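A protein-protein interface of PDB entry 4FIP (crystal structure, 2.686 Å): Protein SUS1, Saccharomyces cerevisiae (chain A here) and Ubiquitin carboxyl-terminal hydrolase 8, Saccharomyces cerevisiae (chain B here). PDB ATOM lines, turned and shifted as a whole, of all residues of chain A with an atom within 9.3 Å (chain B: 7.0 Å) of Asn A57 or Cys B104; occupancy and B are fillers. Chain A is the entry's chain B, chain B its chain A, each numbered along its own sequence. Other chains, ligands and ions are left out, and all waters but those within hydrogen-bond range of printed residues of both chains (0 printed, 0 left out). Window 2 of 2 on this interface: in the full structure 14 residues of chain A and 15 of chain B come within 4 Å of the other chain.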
ATOM      1  N   THR A  46      20.971 -16.714 -19.597  1.00  0.00           N
ATOM      2  CA  THR A  46      19.672 -16.578 -18.981  1.00  0.00           C
ATOM      3  C   THR A  46      19.441 -17.793 -18.121  1.00  0.00           C
ATOM      4  O   THR A  46      19.019 -17.694 -16.989  1.00  0.00           O
ATOM      5  CB  THR A  46      18.570 -16.437 -20.049  1.00  0.00           C
ATOM      6  OG1 THR A  46      18.866 -15.294 -20.847  1.00  0.00           O
ATOM      7  CG2 THR A  46      17.200 -16.251 -19.430  1.00  0.00           C
ATOM      8  N   GLU A  49      21.585 -17.588 -14.910  1.00  0.00           N
ATOM      9  CA  GLU A  49      21.074 -16.618 -13.938  1.00  0.00           C
ATOM     10  C   GLU A  49      19.791 -17.103 -13.292  1.00  0.00           C
ATOM     11  O   GLU A  49      19.557 -16.810 -12.133  1.00  0.00           O
ATOM     12  CB  GLU A  49      20.846 -15.238 -14.544  1.00  0.00           C
ATOM     13  CG  GLU A  49      22.096 -14.589 -15.141  1.00  0.00           C
ATOM     14  CD  GLU A  49      23.202 -14.213 -14.144  1.00  0.00           C
ATOM     15  OE1 GLU A  49      22.910 -13.596 -13.097  1.00  0.00           O
ATOM     16  OE2 GLU A  49      24.388 -14.502 -14.446  1.00  0.00           O
ATOM     17  N   MET A  50      18.969 -17.860 -14.017  1.00  0.00           N
ATOM     18  CA  MET A  50      17.777 -18.458 -13.405  1.00  0.00           C
ATOM     19  C   MET A  50      18.175 -19.422 -12.316  1.00  0.00           C
ATOM     20  O   MET A  50      17.487 -19.559 -11.302  1.00  0.00           O
ATOM     21  CB  MET A  50      16.881 -19.171 -14.424  1.00  0.00           C
ATOM     22  CG  MET A  50      15.950 -18.238 -15.208  1.00  0.00           C
ATOM     23  SD  MET A  50      14.688 -19.027 -16.254  1.00  0.00           S
ATOM     24  CE  MET A  50      15.680 -19.428 -17.687  1.00  0.00           C
ATOM     25  N   ASN A  53      20.053 -17.458  -9.293  1.00  0.00           N
ATOM     26  CA  ASN A  53      19.081 -16.665  -8.513  1.00  0.00           C
ATOM     27  C   ASN A  53      17.802 -17.408  -8.102  1.00  0.00           C
ATOM     28  O   ASN A  53      16.959 -16.834  -7.436  1.00  0.00           O
ATOM     29  CB  ASN A  53      18.737 -15.369  -9.258  1.00  0.00           C
ATOM     30  CG  ASN A  53      19.968 -14.497  -9.509  1.00  0.00           C
ATOM     31  OD1 ASN A  53      20.444 -13.820  -8.620  1.00  0.00           O
ATOM     32  ND2 ASN A  53      20.481 -14.519 -10.718  1.00  0.00           N
ATOM     33  N   GLU A  54      17.677 -18.686  -8.465  1.00  0.00           N
ATOM     34  CA  GLU A  54      16.512 -19.493  -8.093  1.00  0.00           C
ATOM     35  C   GLU A  54      15.190 -18.807  -8.473  1.00  0.00           C
ATOM     36  O   GLU A  54      14.204 -18.864  -7.734  1.00  0.00           O
ATOM     37  CB  GLU A  54      16.519 -19.762  -6.586  1.00  0.00           C
ATOM     38  CG  GLU A  54      17.689 -20.584  -6.079  1.00  0.00           C
ATOM     39  CD  GLU A  54      17.505 -22.061  -6.343  1.00  0.00           C
ATOM     40  OE1 GLU A  54      16.743 -22.689  -5.563  1.00  0.00           O
ATOM     41  OE2 GLU A  54      18.130 -22.582  -7.309  1.00  0.00           O
ATOM     42  N   SER A  55      15.171 -18.156  -9.627  1.00  0.00           N
ATOM     43  CA  SER A  55      14.028 -17.383 -10.025  1.00  0.00           C
ATOM     44  C   SER A  55      13.768 -17.553 -11.496  1.00  0.00           C
ATOM     45  O   SER A  55      14.678 -17.830 -12.248  1.00  0.00           O
ATOM     46  CB  SER A  55      14.281 -15.905  -9.695  1.00  0.00           C
ATOM     47  OG  SER A  55      13.153 -15.070  -9.969  1.00  0.00           O
ATOM     48  N   THR A  56      12.508 -17.395 -11.886  1.00  0.00           N
ATOM     49  CA  THR A  56      12.079 -17.292 -13.301  1.00  0.00           C
ATOM     50  C   THR A  56      11.364 -15.968 -13.596  1.00  0.00           C
ATOM     51  O   THR A  56      10.809 -15.783 -14.680  1.00  0.00           O
ATOM     52  CB  THR A  56      11.108 -18.440 -13.682  1.00  0.00           C
ATOM     53  OG1 THR A  56       9.947 -18.395 -12.838  1.00  0.00           O
ATOM     54  CG2 THR A  56      11.763 -19.778 -13.531  1.00  0.00           C
ATOM     55  N   ASN A  57      11.349 -15.056 -12.627  1.00  0.00           N
ATOM     56  CA  ASN A  57      10.694 -13.758 -12.773  1.00  0.00           C
ATOM     57  C   ASN A  57      11.438 -12.913 -13.801  1.00  0.00           C
ATOM     58  O   ASN A  57      12.618 -12.579 -13.607  1.00  0.00           O
ATOM     59  CB  ASN A  57      10.695 -13.057 -11.431  1.00  0.00           C
ATOM     60  CG  ASN A  57      10.104 -11.675 -11.484  1.00  0.00           C
ATOM     61  OD1 ASN A  57       8.994 -11.492 -11.033  1.00  0.00           O
ATOM     62  ND2 ASN A  57      10.836 -10.698 -12.014  1.00  0.00           N
ATOM     63  N   PHE A  58      10.747 -12.572 -14.892  1.00  0.00           N
ATOM     64  CA  PHE A  58      11.355 -11.832 -16.008  1.00  0.00           C
ATOM     65  C   PHE A  58      12.178 -10.597 -15.588  1.00  0.00           C
ATOM     66  O   PHE A  58      13.343 -10.472 -15.936  1.00  0.00           O
ATOM     67  CB  PHE A  58      10.286 -11.425 -17.023  1.00  0.00           C
ATOM     68  CG  PHE A  58      10.846 -10.661 -18.195  1.00  0.00           C
ATOM     69  CD1 PHE A  58      11.560 -11.311 -19.170  1.00  0.00           C
ATOM     70  CD2 PHE A  58      10.702  -9.285 -18.279  1.00  0.00           C
ATOM     71  CE1 PHE A  58      12.118 -10.619 -20.216  1.00  0.00           C
ATOM     72  CE2 PHE A  58      11.267  -8.575 -19.327  1.00  0.00           C
ATOM     73  CZ  PHE A  58      11.980  -9.250 -20.297  1.00  0.00           C
ATOM     74  N   THR A  59      11.564  -9.692 -14.842  1.00  0.00           N
ATOM     75  CA  THR A  59      12.187  -8.410 -14.533  1.00  0.00           C
ATOM     76  C   THR A  59      13.505  -8.562 -13.796  1.00  0.00           C
ATOM     77  O   THR A  59      14.502  -7.898 -14.098  1.00  0.00           O
ATOM     78  CB  THR A  59      11.258  -7.582 -13.658  1.00  0.00           C
ATOM     79  OG1 THR A  59      10.008  -7.487 -14.322  1.00  0.00           O
ATOM     80  CG2 THR A  59      11.812  -6.186 -13.451  1.00  0.00           C
ATOM     81  N   GLN A  60      13.471  -9.421 -12.796  1.00  0.00           N
ATOM     82  CA  GLN A  60      14.626  -9.711 -11.983  1.00  0.00           C
ATOM     83  C   GLN A  60      15.759 -10.283 -12.827  1.00  0.00           C
ATOM     84  O   GLN A  60      16.902  -9.838 -12.732  1.00  0.00           O
ATOM     85  CB  GLN A  60      14.217 -10.687 -10.873  1.00  0.00           C
ATOM     86  CG  GLN A  60      15.392 -11.302 -10.135  1.00  0.00           C
ATOM     87  CD  GLN A  60      15.028 -11.957  -8.817  1.00  0.00           C
ATOM     88  OE1 GLN A  60      13.855 -11.980  -8.399  1.00  0.00           O
ATOM     89  NE2 GLN A  60      16.047 -12.487  -8.139  1.00  0.00           N
ATOM     90  N   ILE A  61      15.434 -11.270 -13.657  1.00  0.00           N
ATOM     91  CA  ILE A  61      16.445 -11.965 -14.460  1.00  0.00           C
ATOM     92  C   ILE A  61      16.991 -11.042 -15.537  1.00  0.00           C
ATOM     93  O   ILE A  61      18.214 -10.982 -15.748  1.00  0.00           O
ATOM     94  CB  ILE A  61      15.895 -13.293 -15.053  1.00  0.00           C
ATOM     95  CG1 ILE A  61      15.745 -14.335 -13.926  1.00  0.00           C
ATOM     96  CG2 ILE A  61      16.812 -13.873 -16.126  1.00  0.00           C
ATOM     97  CD1 ILE A  61      17.032 -14.775 -13.223  1.00  0.00           C
ATOM     98  N   LEU A  62      16.085 -10.302 -16.186  1.00  0.00           N
ATOM     99  CA  LEU A  62      16.455  -9.293 -17.184  1.00  0.00           C
ATOM    100  C   LEU A  62      17.536  -8.377 -16.682  1.00  0.00           C
ATOM    101  O   LEU A  62      18.469  -8.105 -17.396  1.00  0.00           O
ATOM    102  CB  LEU A  62      15.262  -8.446 -17.576  1.00  0.00           C
ATOM    103  CG  LEU A  62      15.527  -7.476 -18.745  1.00  0.00           C
ATOM    104  CD1 LEU A  62      16.092  -8.185 -19.989  1.00  0.00           C
ATOM    105  CD2 LEU A  62      14.239  -6.710 -19.025  1.00  0.00           C
ATOM    106  N   SER A  63      17.433  -7.966 -15.424  1.00  0.00           N
ATOM    107  CA  SER A  63      18.290  -6.912 -14.898  1.00  0.00           C
ATOM    108  C   SER A  63      19.711  -7.351 -14.726  1.00  0.00           C
ATOM    109  O   SER A  63      20.603  -6.521 -14.686  1.00  0.00           O
ATOM    110  CB  SER A  63      17.760  -6.392 -13.560  1.00  0.00           C
ATOM    111  OG  SER A  63      17.894  -7.377 -12.556  1.00  0.00           O
ATOM    112  N   THR A  64      19.913  -8.652 -14.588  1.00  0.00           N
ATOM    113  CA  THR A  64      21.254  -9.225 -14.482  1.00  0.00           C
ATOM    114  C   THR A  64      21.761  -9.713 -15.854  1.00  0.00           C
ATOM    115  O   THR A  64      22.977  -9.786 -16.079  1.00  0.00           O
ATOM    116  CB  THR A  64      21.268 -10.406 -13.483  1.00  0.00           C
ATOM    117  OG1 THR A  64      20.141 -11.267 -13.746  1.00  0.00           O
ATOM    118  CG2 THR A  64      21.199  -9.888 -12.031  1.00  0.00           C
ATOM    119  N   VAL A  65      20.850 -10.049 -16.763  1.00  0.00           N
ATOM    120  CA  VAL A  65      21.278 -10.576 -18.035  1.00  0.00           C
ATOM    121  C   VAL A  65      21.583  -9.438 -19.001  1.00  0.00           C
ATOM    122  O   VAL A  65      22.537  -9.499 -19.763  1.00  0.00           O
ATOM    123  CB  VAL A  65      20.233 -11.544 -18.656  1.00  0.00           C
ATOM    124  CG1 VAL A  65      20.601 -11.871 -20.089  1.00  0.00           C
ATOM    125  CG2 VAL A  65      20.106 -12.832 -17.861  1.00  0.00           C
ATOM    126  N   ILE B   8       0.774 -18.884  -9.928  1.00  0.00           N
ATOM    127  CA  ILE B   8       0.063 -18.386 -11.103  1.00  0.00           C
ATOM    128  C   ILE B   8      -0.421 -16.954 -10.875  1.00  0.00           C
ATOM    129  O   ILE B   8      -0.915 -16.631  -9.800  1.00  0.00           O
ATOM    130  CB  ILE B   8      -1.193 -19.234 -11.342  1.00  0.00           C
ATOM    131  CG1 ILE B   8      -0.828 -20.687 -11.664  1.00  0.00           C
ATOM    132  CG2 ILE B   8      -2.041 -18.642 -12.447  1.00  0.00           C
ATOM    133  CD1 ILE B   8      -0.348 -20.898 -13.079  1.00  0.00           C
ATOM    134  N   CYS B   9      -0.331 -16.106 -11.888  1.00  0.00           N
ATOM    135  CA  CYS B   9      -0.783 -14.721 -11.752  1.00  0.00           C
ATOM    136  C   CYS B   9      -2.174 -14.638 -11.132  1.00  0.00           C
ATOM    137  O   CYS B   9      -3.143 -14.979 -11.783  1.00  0.00           O
ATOM    138  CB  CYS B   9      -0.817 -14.013 -13.127  1.00  0.00           C
ATOM    139  SG  CYS B   9      -1.449 -12.322 -13.127  1.00  0.00           S
ATOM    140  N   PRO B  10      -2.282 -14.144  -9.895  1.00  0.00           N
ATOM    141  CA  PRO B  10      -3.616 -14.033  -9.259  1.00  0.00           C
ATOM    142  C   PRO B  10      -4.588 -13.100  -9.992  1.00  0.00           C
ATOM    143  O   PRO B  10      -5.801 -13.321  -9.974  1.00  0.00           O
ATOM    144  CB  PRO B  10      -3.318 -13.482  -7.860  1.00  0.00           C
ATOM    145  CG  PRO B  10      -1.918 -12.977  -7.897  1.00  0.00           C
ATOM    146  CD  PRO B  10      -1.227 -13.453  -9.148  1.00  0.00           C
ATOM    147  N   HIS B  11      -4.045 -12.071 -10.635  1.00  0.00           N
ATOM    148  CA  HIS B  11      -4.865 -11.123 -11.393  1.00  0.00           C
ATOM    149  C   HIS B  11      -5.510 -11.794 -12.561  1.00  0.00           C
ATOM    150  O   HIS B  11      -6.698 -11.632 -12.791  1.00  0.00           O
ATOM    151  CB  HIS B  11      -4.021  -9.971 -11.887  1.00  0.00           C
ATOM    152  CG  HIS B  11      -2.920  -9.580 -10.941  1.00  0.00           C
ATOM    153  ND1 HIS B  11      -1.639 -10.018 -11.085  1.00  0.00           N
ATOM    154  CD2 HIS B  11      -2.940  -8.780  -9.814  1.00  0.00           C
ATOM    155  CE1 HIS B  11      -0.886  -9.516 -10.085  1.00  0.00           C
ATOM    156  NE2 HIS B  11      -1.679  -8.765  -9.306  1.00  0.00           N
ATOM    157  N   ILE B  12      -4.751 -12.581 -13.318  1.00  0.00           N
ATOM    158  CA  ILE B  12      -5.353 -13.214 -14.476  1.00  0.00           C
ATOM    159  C   ILE B  12      -6.361 -14.281 -14.022  1.00  0.00           C
ATOM    160  O   ILE B  12      -7.374 -14.476 -14.669  1.00  0.00           O
ATOM    161  CB  ILE B  12      -4.309 -13.749 -15.489  1.00  0.00           C
ATOM    162  CG1 ILE B  12      -4.940 -13.962 -16.877  1.00  0.00           C
ATOM    163  CG2 ILE B  12      -3.703 -15.054 -15.030  1.00  0.00           C
ATOM    164  CD1 ILE B  12      -5.597 -12.734 -17.489  1.00  0.00           C
ATOM    165  N   ILE B  89      -3.656  -3.778 -17.030  1.00  0.00           N
ATOM    166  CA  ILE B  89      -2.371  -4.297 -16.500  1.00  0.00           C
ATOM    167  C   ILE B  89      -1.722  -5.357 -17.365  1.00  0.00           C
ATOM    168  O   ILE B  89      -0.589  -5.764 -17.068  1.00  0.00           O
ATOM    169  CB  ILE B  89      -2.500  -4.892 -15.064  1.00  0.00           C
ATOM    170  CG1 ILE B  89      -3.336  -6.191 -15.082  1.00  0.00           C
ATOM    171  CG2 ILE B  89      -3.066  -3.866 -14.082  1.00  0.00           C
ATOM    172  CD1 ILE B  89      -3.738  -6.683 -13.704  1.00  0.00           C
ATOM    173  N   PHE B 100       2.139 -10.463 -20.710  1.00  0.00           N
ATOM    174  CA  PHE B 100       2.889  -9.965 -19.547  1.00  0.00           C
ATOM    175  C   PHE B 100       1.916  -9.368 -18.548  1.00  0.00           C
ATOM    176  O   PHE B 100       0.908  -8.808 -18.958  1.00  0.00           O
ATOM    177  CB  PHE B 100       3.913  -8.909 -19.978  1.00  0.00           C
ATOM    178  CG  PHE B 100       4.926  -8.554 -18.911  1.00  0.00           C
ATOM    179  CD1 PHE B 100       6.090  -9.275 -18.767  1.00  0.00           C
ATOM    180  CD2 PHE B 100       4.716  -7.502 -18.052  1.00  0.00           C
ATOM    181  CE1 PHE B 100       7.017  -8.941 -17.795  1.00  0.00           C
ATOM    182  CE2 PHE B 100       5.640  -7.170 -17.084  1.00  0.00           C
ATOM    183  CZ  PHE B 100       6.794  -7.881 -16.957  1.00  0.00           C
ATOM    184  N   CYS B 101       2.209  -9.478 -17.251  1.00  0.00           N
ATOM    185  CA  CYS B 101       1.358  -8.857 -16.197  1.00  0.00           C
ATOM    186  C   CYS B 101       2.167  -7.776 -15.551  1.00  0.00           C
ATOM    187  O   CYS B 101       3.195  -8.071 -14.937  1.00  0.00           O
ATOM    188  CB  CYS B 101       0.898  -9.875 -15.117  1.00  0.00           C
ATOM    189  SG  CYS B 101       0.091  -9.094 -13.705  1.00  0.00           S
ATOM    190  N   PHE B 102       1.731  -6.535 -15.677  1.00  0.00           N
ATOM    191  CA  PHE B 102       2.539  -5.420 -15.143  1.00  0.00           C
ATOM    192  C   PHE B 102       2.363  -5.143 -13.648  1.00  0.00           C
ATOM    193  O   PHE B 102       3.069  -4.301 -13.093  1.00  0.00           O
ATOM    194  CB  PHE B 102       2.350  -4.147 -15.968  1.00  0.00           C
ATOM    195  CG  PHE B 102       2.957  -4.232 -17.336  1.00  0.00           C
ATOM    196  CD1 PHE B 102       2.287  -4.845 -18.367  1.00  0.00           C
ATOM    197  CD2 PHE B 102       4.203  -3.727 -17.577  1.00  0.00           C
ATOM    198  CE1 PHE B 102       2.839  -4.943 -19.617  1.00  0.00           C
ATOM    199  CE2 PHE B 102       4.766  -3.814 -18.836  1.00  0.00           C
ATOM    200  CZ  PHE B 102       4.083  -4.437 -19.853  1.00  0.00           C
ATOM    201  N   LYS B 103       1.451  -5.865 -13.004  1.00  0.00           N
ATOM    202  CA  LYS B 103       1.413  -5.889 -11.544  1.00  0.00           C
ATOM    203  C   LYS B 103       2.288  -7.009 -10.997  1.00  0.00           C
ATOM    204  O   LYS B 103       2.982  -6.798 -10.026  1.00  0.00           O
ATOM    205  CB  LYS B 103      -0.005  -6.012 -11.001  1.00  0.00           C
ATOM    206  CG  LYS B 103      -0.791  -4.724 -11.091  1.00  0.00           C
ATOM    207  CD  LYS B 103      -2.139  -4.863 -10.403  1.00  0.00           C
ATOM    208  CE  LYS B 103      -2.607  -3.572  -9.742  1.00  0.00           C
ATOM    209  NZ  LYS B 103      -3.380  -3.967  -8.527  1.00  0.00           N
ATOM    210  N   CYS B 104       2.267  -8.194 -11.607  1.00  0.00           N
ATOM    211  CA  CYS B 104       3.226  -9.236 -11.233  1.00  0.00           C
ATOM    212  C   CYS B 104       4.640  -8.920 -11.674  1.00  0.00           C
ATOM    213  O   CYS B 104       5.552  -9.607 -11.265  1.00  0.00           O
ATOM    214  CB  CYS B 104       2.855 -10.569 -11.861  1.00  0.00           C
ATOM    215  SG  CYS B 104       1.475 -11.366 -11.056  1.00  0.00           S
ATOM    216  N   GLU B 105       4.821  -7.936 -12.553  1.00  0.00           N
ATOM    217  CA  GLU B 105       6.120  -7.666 -13.174  1.00  0.00           C
ATOM    218  C   GLU B 105       6.747  -8.890 -13.861  1.00  0.00           C
ATOM    219  O   GLU B 105       7.943  -9.016 -13.893  1.00  0.00           O
ATOM    220  CB  GLU B 105       7.099  -7.112 -12.128  1.00  0.00           C
ATOM    221  CG  GLU B 105       6.743  -5.724 -11.612  1.00  0.00           C
ATOM    222  CD  GLU B 105       7.972  -4.952 -11.125  1.00  0.00           C
ATOM    223  OE1 GLU B 105       8.160  -3.774 -11.524  1.00  0.00           O
ATOM    224  OE2 GLU B 105       8.762  -5.528 -10.344  1.00  0.00           O
ATOM    225  N   ASP B 106       5.936  -9.781 -14.415  1.00  0.00           N
ATOM    226  CA  ASP B 106       6.428 -11.051 -14.966  1.00  0.00           C
ATOM    227  C   ASP B 106       5.459 -11.566 -16.046  1.00  0.00           C
ATOM    228  O   ASP B 106       4.344 -11.055 -16.129  1.00  0.00           O
ATOM    229  CB  ASP B 106       6.560 -12.076 -13.817  1.00  0.00           C
ATOM    230  CG  ASP B 106       7.364 -13.334 -14.197  1.00  0.00           C
ATOM    231  OD1 ASP B 106       8.209 -13.327 -15.116  1.00  0.00           O
ATOM    232  OD2 ASP B 106       7.151 -14.350 -13.534  1.00  0.00           O
ATOM    233  N   TYR B 107       5.887 -12.522 -16.878  1.00  0.00           N
ATOM    234  CA  TYR B 107       5.022 -13.132 -17.904  1.00  0.00           C
ATOM    235  C   TYR B 107       4.151 -14.267 -17.318  1.00  0.00           C
ATOM    236  O   TYR B 107       4.540 -14.984 -16.355  1.00  0.00           O
ATOM    237  CB  TYR B 107       5.843 -13.702 -19.088  1.00  0.00           C
ATOM    238  CG  TYR B 107       6.479 -12.661 -20.020  1.00  0.00           C
ATOM    239  CD1 TYR B 107       5.750 -12.081 -21.050  1.00  0.00           C
ATOM    240  CD2 TYR B 107       7.798 -12.272 -19.883  1.00  0.00           C
ATOM    241  CE1 TYR B 107       6.306 -11.135 -21.881  1.00  0.00           C
ATOM    242  CE2 TYR B 107       8.346 -11.330 -20.726  1.00  0.00           C
ATOM    243  CZ  TYR B 107       7.594 -10.776 -21.724  1.00  0.00           C
ATOM    244  OH  TYR B 107       8.122  -9.832 -22.560  1.00  0.00           O
ATOM    245  N   ILE B 108       2.980 -14.427 -17.919  1.00  0.00           N
ATOM    246  CA  ILE B 108       2.099 -15.523 -17.618  1.00  0.00           C
ATOM    247  C   ILE B 108       2.416 -16.617 -18.621  1.00  0.00           C
ATOM    248  O   ILE B 108       1.787 -16.708 -19.692  1.00  0.00           O
ATOM    249  CB  ILE B 108       0.631 -15.086 -17.745  1.00  0.00           C
ATOM    250  CG1 ILE B 108       0.354 -13.868 -16.841  1.00  0.00           C
ATOM    251  CG2 ILE B 108      -0.328 -16.222 -17.391  1.00  0.00           C
ATOM    252  CD1 ILE B 108      -0.992 -13.207 -17.106  1.00  0.00           C
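O of Glu B105 lies within hydrogen-bond range of OG1 of Thr A59. The side-chain carboxylate (OD1) of Asp B106 sits at hydrogen-bond distance from the backbone NH (N) of Phe A58 (2.7 Å).
N of Cys B101 sits at hydrogen-bond distance from O of Asp B106 (2.9 Å). The side-chain hydroxyl (OG) of Ser A55 sits at hydrogen-bond distance from the backbone NH (N) of Asn A57, 3.2 Å away. The side-chain amide nitrogen (ND2) of Asn A57 sits close to the backbone NH (N) of Thr A59 (3.1 Å). The side-chain amide nitrogen (ND2) of Asn A57 lies close to the backbone NH (N) of Gln A60 (3.0 Å).
Thr A56 touches Asp B106 (O to OD1, 3.6 Å). Cys B104 touches Asn A57 (O to OD1, 3.9 Å). Asn A57 touches Glu B105 (ND2 to O, 3.8 Å). Asn A57 touches Asp B106 (CA to OD1, 3.4 Å). CD2 of Phe A58 touches CE1 of Phe B100 (3.7 Å). CD1 of Phe A58 touches CE2 of Tyr B107, at 3.6 Å.
Of the printed residues of chain B, Thr A56 touches Asp B106 (3.6 Å). Of chain B, only Cys B104, Glu B105 and Asp B106 come within 4 Å of Asn A57. Of the printed residues of chain B, Phe A58 touches Phe B100, Asp B106 and Tyr B107. Of the printed residues of chain B, Thr A59 touches Glu B105 (2.6 Å). Cys B104 touches just one residue of chain A: Asn A57 (3.9 Å). Of the printed residues of chain A, Glu B105 touches Asn A57 (3.8 Å) and Thr A59 (2.6 Å). Asp B106 touches just these residues of chain A: Thr A56, Asn A57 and Phe A58. Of the printed residues of chain A, Tyr B107 touches Phe A58. The nearest residue of chain A that does not touch Cys B104 is Thr A59 (5.8 Å). The nearest printed residue of chain B that does not touch Phe A58 is Glu B105 (4.6 Å).
Hydrophobic or aromatic side chains of chain B that line the printed part of chain A: Phe B100 and Tyr B107. Of the 16 printed residues of chain A, 4 touch a printed residue of chain B. Hydrophobic or aromatic side chains of chain A within 4 Å of the printed part of chain B: Phe A58. Among the printed residues, 8 pairs touch across the chains. Among the printed residues, no Asp or Glu carboxylate lies within 4 Å of a Lys or Arg side-chain nitrogen of the other chain.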
